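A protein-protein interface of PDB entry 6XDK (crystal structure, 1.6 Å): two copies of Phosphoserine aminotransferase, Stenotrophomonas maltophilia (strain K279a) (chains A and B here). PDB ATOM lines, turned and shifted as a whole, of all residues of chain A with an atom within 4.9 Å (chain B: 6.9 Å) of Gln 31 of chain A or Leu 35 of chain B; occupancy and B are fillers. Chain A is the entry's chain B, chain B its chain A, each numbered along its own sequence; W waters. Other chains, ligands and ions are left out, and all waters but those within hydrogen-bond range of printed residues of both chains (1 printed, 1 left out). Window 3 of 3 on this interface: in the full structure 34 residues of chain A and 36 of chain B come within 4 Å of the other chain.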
ATOM      1  N   LEU A  27      -6.442  -4.542 -29.840  1.00  0.00           N
ATOM      2  CA  LEU A  27      -6.238  -3.188 -29.346  1.00  0.00           C
ATOM      3  C   LEU A  27      -6.140  -2.172 -30.482  1.00  0.00           C
ATOM      4  O   LEU A  27      -6.693  -1.071 -30.385  1.00  0.00           O
ATOM      5  CB  LEU A  27      -4.964  -3.136 -28.507  1.00  0.00           C
ATOM      6  CG  LEU A  27      -5.055  -3.878 -27.184  1.00  0.00           C
ATOM      7  CD1 LEU A  27      -3.668  -3.948 -26.538  1.00  0.00           C
ATOM      8  CD2 LEU A  27      -6.040  -3.135 -26.325  1.00  0.00           C
ATOM      9  N   ARG A  28      -5.398  -2.512 -31.540  1.00  0.00           N
ATOM     10  CA  ARG A  28      -5.284  -1.601 -32.673  1.00  0.00           C
ATOM     11  C   ARG A  28      -6.642  -1.331 -33.310  1.00  0.00           C
ATOM     12  O   ARG A  28      -6.927  -0.191 -33.699  1.00  0.00           O
ATOM     13  CB  ARG A  28      -4.299  -2.155 -33.704  1.00  0.00           C
ATOM     14  CG  ARG A  28      -2.843  -1.798 -33.410  1.00  0.00           C
ATOM     15  CD  ARG A  28      -1.889  -2.282 -34.509  1.00  0.00           C
ATOM     16  NE  ARG A  28      -1.480  -3.681 -34.345  1.00  0.00           N
ATOM     17  CZ  ARG A  28      -1.953  -4.703 -35.062  1.00  0.00           C
ATOM     18  NH1 ARG A  28      -2.868  -4.504 -36.012  1.00  0.00           N
ATOM     19  NH2 ARG A  28      -1.507  -5.931 -34.833  1.00  0.00           N
ATOM     20  N   GLN A  29      -7.489  -2.362 -33.434  1.00  0.00           N
ATOM     21  CA  GLN A  29      -8.800  -2.161 -34.049  1.00  0.00           C
ATOM     22  C   GLN A  29      -9.693  -1.296 -33.177  1.00  0.00           C
ATOM     23  O   GLN A  29     -10.372  -0.381 -33.673  1.00  0.00           O
ATOM     24  CB  GLN A  29      -9.483  -3.506 -34.316  1.00  0.00           C
ATOM     25  CG  GLN A  29     -10.849  -3.332 -34.957  1.00  0.00           C
ATOM     26  CD  GLN A  29     -11.466  -4.644 -35.403  1.00  0.00           C
ATOM     27  OE1 GLN A  29     -10.845  -5.707 -35.328  1.00  0.00           O
ATOM     28  NE2 GLN A  29     -12.707  -4.575 -35.869  1.00  0.00           N
ATOM     29  N   ALA A  30      -9.700  -1.560 -31.872  1.00  0.00           N
ATOM     30  CA  ALA A  30     -10.519  -0.769 -30.963  1.00  0.00           C
ATOM     31  C   ALA A  30     -10.112   0.695 -30.984  1.00  0.00           C
ATOM     32  O   ALA A  30     -10.974   1.579 -30.967  1.00  0.00           O
ATOM     33  CB  ALA A  30     -10.430  -1.330 -29.547  1.00  0.00           C
ATOM     34  N   GLN A  31      -8.810   0.976 -31.019  1.00  0.00           N
ATOM     35  CA  GLN A  31      -8.371   2.357 -31.159  1.00  0.00           C
ATOM     36  C   GLN A  31      -8.825   2.956 -32.487  1.00  0.00           C
ATOM     37  O   GLN A  31      -9.318   4.090 -32.531  1.00  0.00           O
ATOM     38  CB  GLN A  31      -6.860   2.459 -31.041  1.00  0.00           C
ATOM     39  CG  GLN A  31      -6.414   3.901 -31.226  1.00  0.00           C
ATOM     40  CD  GLN A  31      -4.942   4.049 -31.174  1.00  0.00           C
ATOM     41  OE1 GLN A  31      -4.220   3.284 -31.807  1.00  0.00           O
ATOM     42  NE2 GLN A  31      -4.465   5.037 -30.415  1.00  0.00           N
ATOM     43  N   ALA A  32      -8.648   2.213 -33.588  1.00  0.00           N
ATOM     44  CA  ALA A  32      -8.858   2.802 -34.907  1.00  0.00           C
ATOM     45  C   ALA A  32     -10.308   3.202 -35.114  1.00  0.00           C
ATOM     46  O   ALA A  32     -10.586   4.247 -35.707  1.00  0.00           O
ATOM     47  CB  ALA A  32      -8.407   1.840 -36.006  1.00  0.00           C
ATOM     48  N   GLU A  33     -11.255   2.399 -34.634  1.00  0.00           N
ATOM     49  CA  GLU A  33     -12.654   2.703 -34.895  1.00  0.00           C
ATOM     50  C   GLU A  33     -13.372   3.255 -33.670  1.00  0.00           C
ATOM     51  O   GLU A  33     -14.605   3.211 -33.614  1.00  0.00           O
ATOM     52  CB  GLU A  33     -13.381   1.482 -35.455  1.00  0.00           C
ATOM     53  CG  GLU A  33     -13.421   0.300 -34.562  1.00  0.00           C
ATOM     54  CD  GLU A  33     -14.056  -0.930 -35.239  1.00  0.00           C
ATOM     55  OE1 GLU A  33     -14.409  -0.849 -36.443  1.00  0.00           O
ATOM     56  OE2 GLU A  33     -14.203  -1.977 -34.567  1.00  0.00           O
ATOM     57  N   MET A  34     -12.630   3.819 -32.702  1.00  0.00           N
ATOM     58  CA  MET A  34     -13.255   4.330 -31.486  1.00  0.00           C
ATOM     59  C   MET A  34     -14.126   5.550 -31.750  1.00  0.00           C
ATOM     60  O   MET A  34     -15.003   5.851 -30.946  1.00  0.00           O
ATOM     61  CB  MET A  34     -12.195   4.688 -30.446  1.00  0.00           C
ATOM     62  CG  MET A  34     -12.709   4.645 -29.010  1.00  0.00           C
ATOM     63  SD  MET A  34     -11.735   5.714 -27.945  1.00  0.00           S
ATOM     64  CE  MET A  34     -12.878   5.894 -26.581  1.00  0.00           C
ATOM     65  N   ALA B  30      -9.027  10.162 -25.279  1.00  0.00           N
ATOM     66  CA  ALA B  30      -9.047   8.734 -24.972  1.00  0.00           C
ATOM     67  C   ALA B  30      -8.551   7.913 -26.151  1.00  0.00           C
ATOM     68  O   ALA B  30      -7.780   6.971 -25.965  1.00  0.00           O
ATOM     69  CB  ALA B  30     -10.455   8.288 -24.550  1.00  0.00           C
ATOM     70  N   GLN B  31      -9.010   8.225 -27.366  1.00  0.00           N
ATOM     71  CA  GLN B  31      -8.522   7.512 -28.543  1.00  0.00           C
ATOM     72  C   GLN B  31      -7.026   7.691 -28.721  1.00  0.00           C
ATOM     73  O   GLN B  31      -6.299   6.722 -28.982  1.00  0.00           O
ATOM     74  CB  GLN B  31      -9.234   7.990 -29.803  1.00  0.00           C
ATOM     75  CG  GLN B  31      -8.608   7.376 -31.076  1.00  0.00           C
ATOM     76  CD  GLN B  31      -9.294   7.843 -32.319  1.00  0.00           C
ATOM     77  OE1 GLN B  31      -9.609   9.021 -32.452  1.00  0.00           O
ATOM     78  NE2 GLN B  31      -9.577   6.916 -33.229  1.00  0.00           N
ATOM     79  N   ALA B  32      -6.545   8.928 -28.582  1.00  0.00           N
ATOM     80  CA  ALA B  32      -5.154   9.211 -28.878  1.00  0.00           C
ATOM     81  C   ALA B  32      -4.225   8.496 -27.916  1.00  0.00           C
ATOM     82  O   ALA B  32      -3.164   8.004 -28.320  1.00  0.00           O
ATOM     83  CB  ALA B  32      -4.904  10.717 -28.840  1.00  0.00           C
ATOM     84  N   GLU B  33      -4.594   8.409 -26.642  1.00  0.00           N
ATOM     85  CA  GLU B  33      -3.635   7.787 -25.741  1.00  0.00           C
ATOM     86  C   GLU B  33      -4.021   6.362 -25.350  1.00  0.00           C
ATOM     87  O   GLU B  33      -3.399   5.788 -24.443  1.00  0.00           O
ATOM     88  CB  GLU B  33      -3.383   8.668 -24.520  1.00  0.00           C
ATOM     89  CG  GLU B  33      -4.560   9.101 -23.705  1.00  0.00           C
ATOM     90  CD  GLU B  33      -4.109   9.828 -22.446  1.00  0.00           C
ATOM     91  OE1 GLU B  33      -4.966  10.184 -21.582  1.00  0.00           O
ATOM     92  OE2 GLU B  33      -2.868  10.022 -22.327  1.00  0.00           O
ATOM     93  N   MET B  34      -4.940   5.734 -26.101  1.00  0.00           N
ATOM     94  CA  MET B  34      -5.373   4.384 -25.746  1.00  0.00           C
ATOM     95  C   MET B  34      -4.195   3.425 -25.663  1.00  0.00           C
ATOM     96  O   MET B  34      -4.153   2.567 -24.777  1.00  0.00           O
ATOM     97  CB  MET B  34      -6.403   3.850 -26.741  1.00  0.00           C
ATOM     98  CG  MET B  34      -7.019   2.531 -26.269  1.00  0.00           C
ATOM     99  SD  MET B  34      -8.323   1.876 -27.314  1.00  0.00           S
ATOM    100  CE  MET B  34      -9.535   3.177 -27.162  1.00  0.00           C
ATOM    101  N   LEU B  35      -3.236   3.550 -26.573  1.00  0.00           N
ATOM    102  CA  LEU B  35      -2.082   2.664 -26.585  1.00  0.00           C
ATOM    103  C   LEU B  35      -0.817   3.357 -26.126  1.00  0.00           C
ATOM    104  O   LEU B  35       0.283   2.818 -26.314  1.00  0.00           O
ATOM    105  CB  LEU B  35      -1.891   2.068 -27.980  1.00  0.00           C
ATOM    106  CG  LEU B  35      -3.202   1.423 -28.443  1.00  0.00           C
ATOM    107  CD1 LEU B  35      -3.055   0.865 -29.840  1.00  0.00           C
ATOM    108  CD2 LEU B  35      -3.627   0.327 -27.471  1.00  0.00           C
ATOM    109  N   ASP B  36      -0.942   4.541 -25.535  1.00  0.00           N
ATOM    110  CA  ASP B  36       0.215   5.378 -25.284  1.00  0.00           C
ATOM    111  C   ASP B  36      -0.128   6.409 -24.215  1.00  0.00           C
ATOM    112  O   ASP B  36      -0.027   7.617 -24.462  1.00  0.00           O
ATOM    113  CB  ASP B  36       0.642   6.065 -26.587  1.00  0.00           C
ATOM    114  CG  ASP B  36       1.994   6.737 -26.494  1.00  0.00           C
ATOM    115  OD1 ASP B  36       2.741   6.502 -25.514  1.00  0.00           O
ATOM    116  OD2 ASP B  36       2.302   7.524 -27.410  1.00  0.00           O
ATOM    117  N   TRP B  37      -0.533   5.940 -23.043  1.00  0.00           N
ATOM    118  CA  TRP B  37      -0.960   6.830 -21.975  1.00  0.00           C
ATOM    119  C   TRP B  37       0.187   7.728 -21.527  1.00  0.00           C
ATOM    120  O   TRP B  37       1.246   7.241 -21.123  1.00  0.00           O
ATOM    121  CB  TRP B  37      -1.473   6.012 -20.801  1.00  0.00           C
ATOM    122  CG  TRP B  37      -1.932   6.839 -19.638  1.00  0.00           C
ATOM    123  CD1 TRP B  37      -3.159   7.435 -19.477  1.00  0.00           C
ATOM    124  CD2 TRP B  37      -1.201   7.100 -18.440  1.00  0.00           C
ATOM    125  NE1 TRP B  37      -3.216   8.071 -18.255  1.00  0.00           N
ATOM    126  CE2 TRP B  37      -2.028   7.868 -17.599  1.00  0.00           C
ATOM    127  CE3 TRP B  37       0.072   6.743 -17.990  1.00  0.00           C
ATOM    128  CZ2 TRP B  37      -1.615   8.309 -16.343  1.00  0.00           C
ATOM    129  CZ3 TRP B  37       0.480   7.177 -16.743  1.00  0.00           C
ATOM    130  CH2 TRP B  37      -0.363   7.962 -15.939  1.00  0.00           C
ATOM    131  N   SER B  40       3.795   7.083 -22.476  1.00  0.00           N
ATOM    132  CA  SER B  40       4.463   5.947 -21.842  1.00  0.00           C
ATOM    133  C   SER B  40       4.529   4.707 -22.720  1.00  0.00           C
ATOM    134  O   SER B  40       5.287   3.789 -22.397  1.00  0.00           O
ATOM    135  CB  SER B  40       3.751   5.591 -20.530  1.00  0.00           C
ATOM    136  OG  SER B  40       2.501   4.929 -20.743  1.00  0.00           O
ATOM    137  N   GLY B  41       3.754   4.647 -23.800  1.00  0.00           N
ATOM    138  CA  GLY B  41       3.651   3.443 -24.602  1.00  0.00           C
ATOM    139  C   GLY B  41       2.801   2.353 -23.993  1.00  0.00           C
ATOM    140  O   GLY B  41       2.755   1.237 -24.531  1.00  0.00           O
ATOM    141  N   ALA B  42       2.146   2.631 -22.878  1.00  0.00           N
ATOM    142  CA  ALA B  42       1.339   1.648 -22.171  1.00  0.00           C
ATOM    143  C   ALA B  42      -0.137   1.929 -22.411  1.00  0.00           C
ATOM    144  O   ALA B  42      -0.545   3.086 -22.538  1.00  0.00           O
ATOM    145  CB  ALA B  42       1.632   1.701 -20.670  1.00  0.00           C
ATOM    146  N   SER B  43      -0.951   0.878 -22.468  1.00  0.00           N
ATOM    147  CA  SER B  43      -2.389   1.080 -22.611  1.00  0.00           C
ATOM    148  C   SER B  43      -3.064   1.059 -21.253  1.00  0.00           C
ATOM    149  O   SER B  43      -2.752   0.221 -20.404  1.00  0.00           O
ATOM    150  CB  SER B  43      -3.047   0.030 -23.507  1.00  0.00           C
ATOM    151  OG  SER B  43      -4.471   0.215 -23.516  1.00  0.00           O
ATOM    152  N   ILE B  44      -4.003   1.990 -21.060  1.00  0.00           N
ATOM    153  CA  ILE B  44      -4.813   1.997 -19.841  1.00  0.00           C
ATOM    154  C   ILE B  44      -5.516   0.653 -19.664  1.00  0.00           C
ATOM    155  O   ILE B  44      -5.629   0.141 -18.537  1.00  0.00           O
ATOM    156  CB  ILE B  44      -5.847   3.156 -19.851  1.00  0.00           C
ATOM    157  CG1 ILE B  44      -5.194   4.492 -19.508  1.00  0.00           C
ATOM    158  CG2 ILE B  44      -6.930   2.905 -18.820  1.00  0.00           C
ATOM    159  CD1 ILE B  44      -5.041   4.757 -18.006  1.00  0.00           C
ATOM    160  N   VAL B  45      -5.972   0.043 -20.764  1.00  0.00           N
ATOM    161  CA  VAL B  45      -6.769  -1.172 -20.586  1.00  0.00           C
ATOM    162  C   VAL B  45      -5.918  -2.330 -20.100  1.00  0.00           C
ATOM    163  O   VAL B  45      -6.469  -3.320 -19.617  1.00  0.00           O
ATOM    164  CB  VAL B  45      -7.540  -1.629 -21.846  1.00  0.00           C
ATOM    165  CG1 VAL B  45      -8.392  -0.485 -22.433  1.00  0.00           C
ATOM    166  CG2 VAL B  45      -6.607  -2.262 -22.874  1.00  0.00           C
ATOM    167  N   GLU B  46      -4.594  -2.239 -20.171  1.00  0.00           N
ATOM    168  CA  GLU B  46      -3.758  -3.330 -19.671  1.00  0.00           C
ATOM    169  C   GLU B  46      -3.032  -2.973 -18.376  1.00  0.00           C
ATOM    170  O   GLU B  46      -2.209  -3.765 -17.909  1.00  0.00           O
ATOM    171  CB  GLU B  46      -2.765  -3.767 -20.752  1.00  0.00           C
ATOM    172  CG  GLU B  46      -3.423  -4.548 -21.916  1.00  0.00           C
ATOM    173  CD  GLU B  46      -2.493  -4.736 -23.125  1.00  0.00           C
ATOM    174  OE1 GLU B  46      -1.921  -3.731 -23.612  1.00  0.00           O
ATOM    175  OE2 GLU B  46      -2.291  -5.882 -23.577  1.00  0.00           O
HETATM  176  O   HOH W   1     -12.256   6.140 -34.994  1.00  0.00           O
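Gln 31 of chain A touches its own counterpart, Gln 31 of chain B. Gln 31 of chain A touches Ala 32 of chain B, and with the chains exchanged Ala 32 of chain A touches Gln 31 of chain B. Gln 31 of chain A touches Met 34 of chain B, and with the chains exchanged Met 34 of chain A touches Gln 31 of chain B. Met 34 of chain A touches Ala 30 of chain B, but with the chains exchanged Ala 30 of chain A does not touch Met 34 of chain B (4.3 Å). 5 positions are printed for both chains.
Water W1 lies within hydrogen-bond range of the backbone carbonyl oxygen of Ala 32 of chain A, the backbone NH of Met 34 of chain A and the side-chain amide nitrogen of Gln 31 of chain B.
Hydrophobic or aromatic side chains of chain B that line the printed part of chain A: Ala 30, Met 34, Leu 35 and Val 45. Of the 8 printed residues of chain A, 4 touch a printed residue of chain B. Printed residues of chain A that touch a printed residue of chain B: Leu 27, Gln 31, Ala 32 and Met 34. Hydrophobic or aromatic side chains of chain A that line the printed part of chain B: Leu 27 and Met 34. Among the printed residues, no Asp or Glu carboxylate lies within 4 Å of a Lys or Arg side-chain nitrogen of the other chain.
O of Met 34 of chain B sits at hydrogen-bond distance from OG of Ser 43 of chain B. The side-chain hydroxyl (OG) of Ser 43 of chain B sits close to the backbone NH (N) of Val 45 of chain B (3.1 Å).
O of Gln 31 of chain B is in hydrogen-bond range of NE2 of Gln 31 of chain A. The backbone NH (N) of Gln 31 of chain B sits close to the side-chain sulfur (SD) of Met 34 of chain A (3.8 Å).
Among the printed residues, pairs that only touch across the chains: Gln 31 of chain A with Leu 35 of chain B, Leu 27 of chain A with Glu 46 of chain B, Met 34 of chain A with Met 34 of chain B, Leu 27 of chain A with Val 45 of chain B, Ala 32 of chain A with Gln 31 of chain B, Gln 31 of chain A with Met 34 of chain B, Leu 27 of chain A with Leu 35 of chain B, Gln 31 of chain A with Ala 32 of chain B and Met 34 of chain A with Ala 30 of chain B.
Leu 35 of chain B touches just these residues of chain A: Leu 27 and Gln 31. Of the printed residues of chain A, Ala 30 of chain B touches Met 34. Of the printed residues of chain B, Ala 32 of chain A touches Gln 31 (3.8 Å). Of the printed residues of chain A, Ala 32 of chain B touches Gln 31. Of the printed residues of chain A, Gln 31 of chain B touches Gln 31, Ala 32 and Met 34. Arg 28 of chain A touches none of the printed residues of chain B. The nearest printed residue of chain A that does not touch Leu 35 of chain B is Arg 28 of chain A (4.4 Å).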
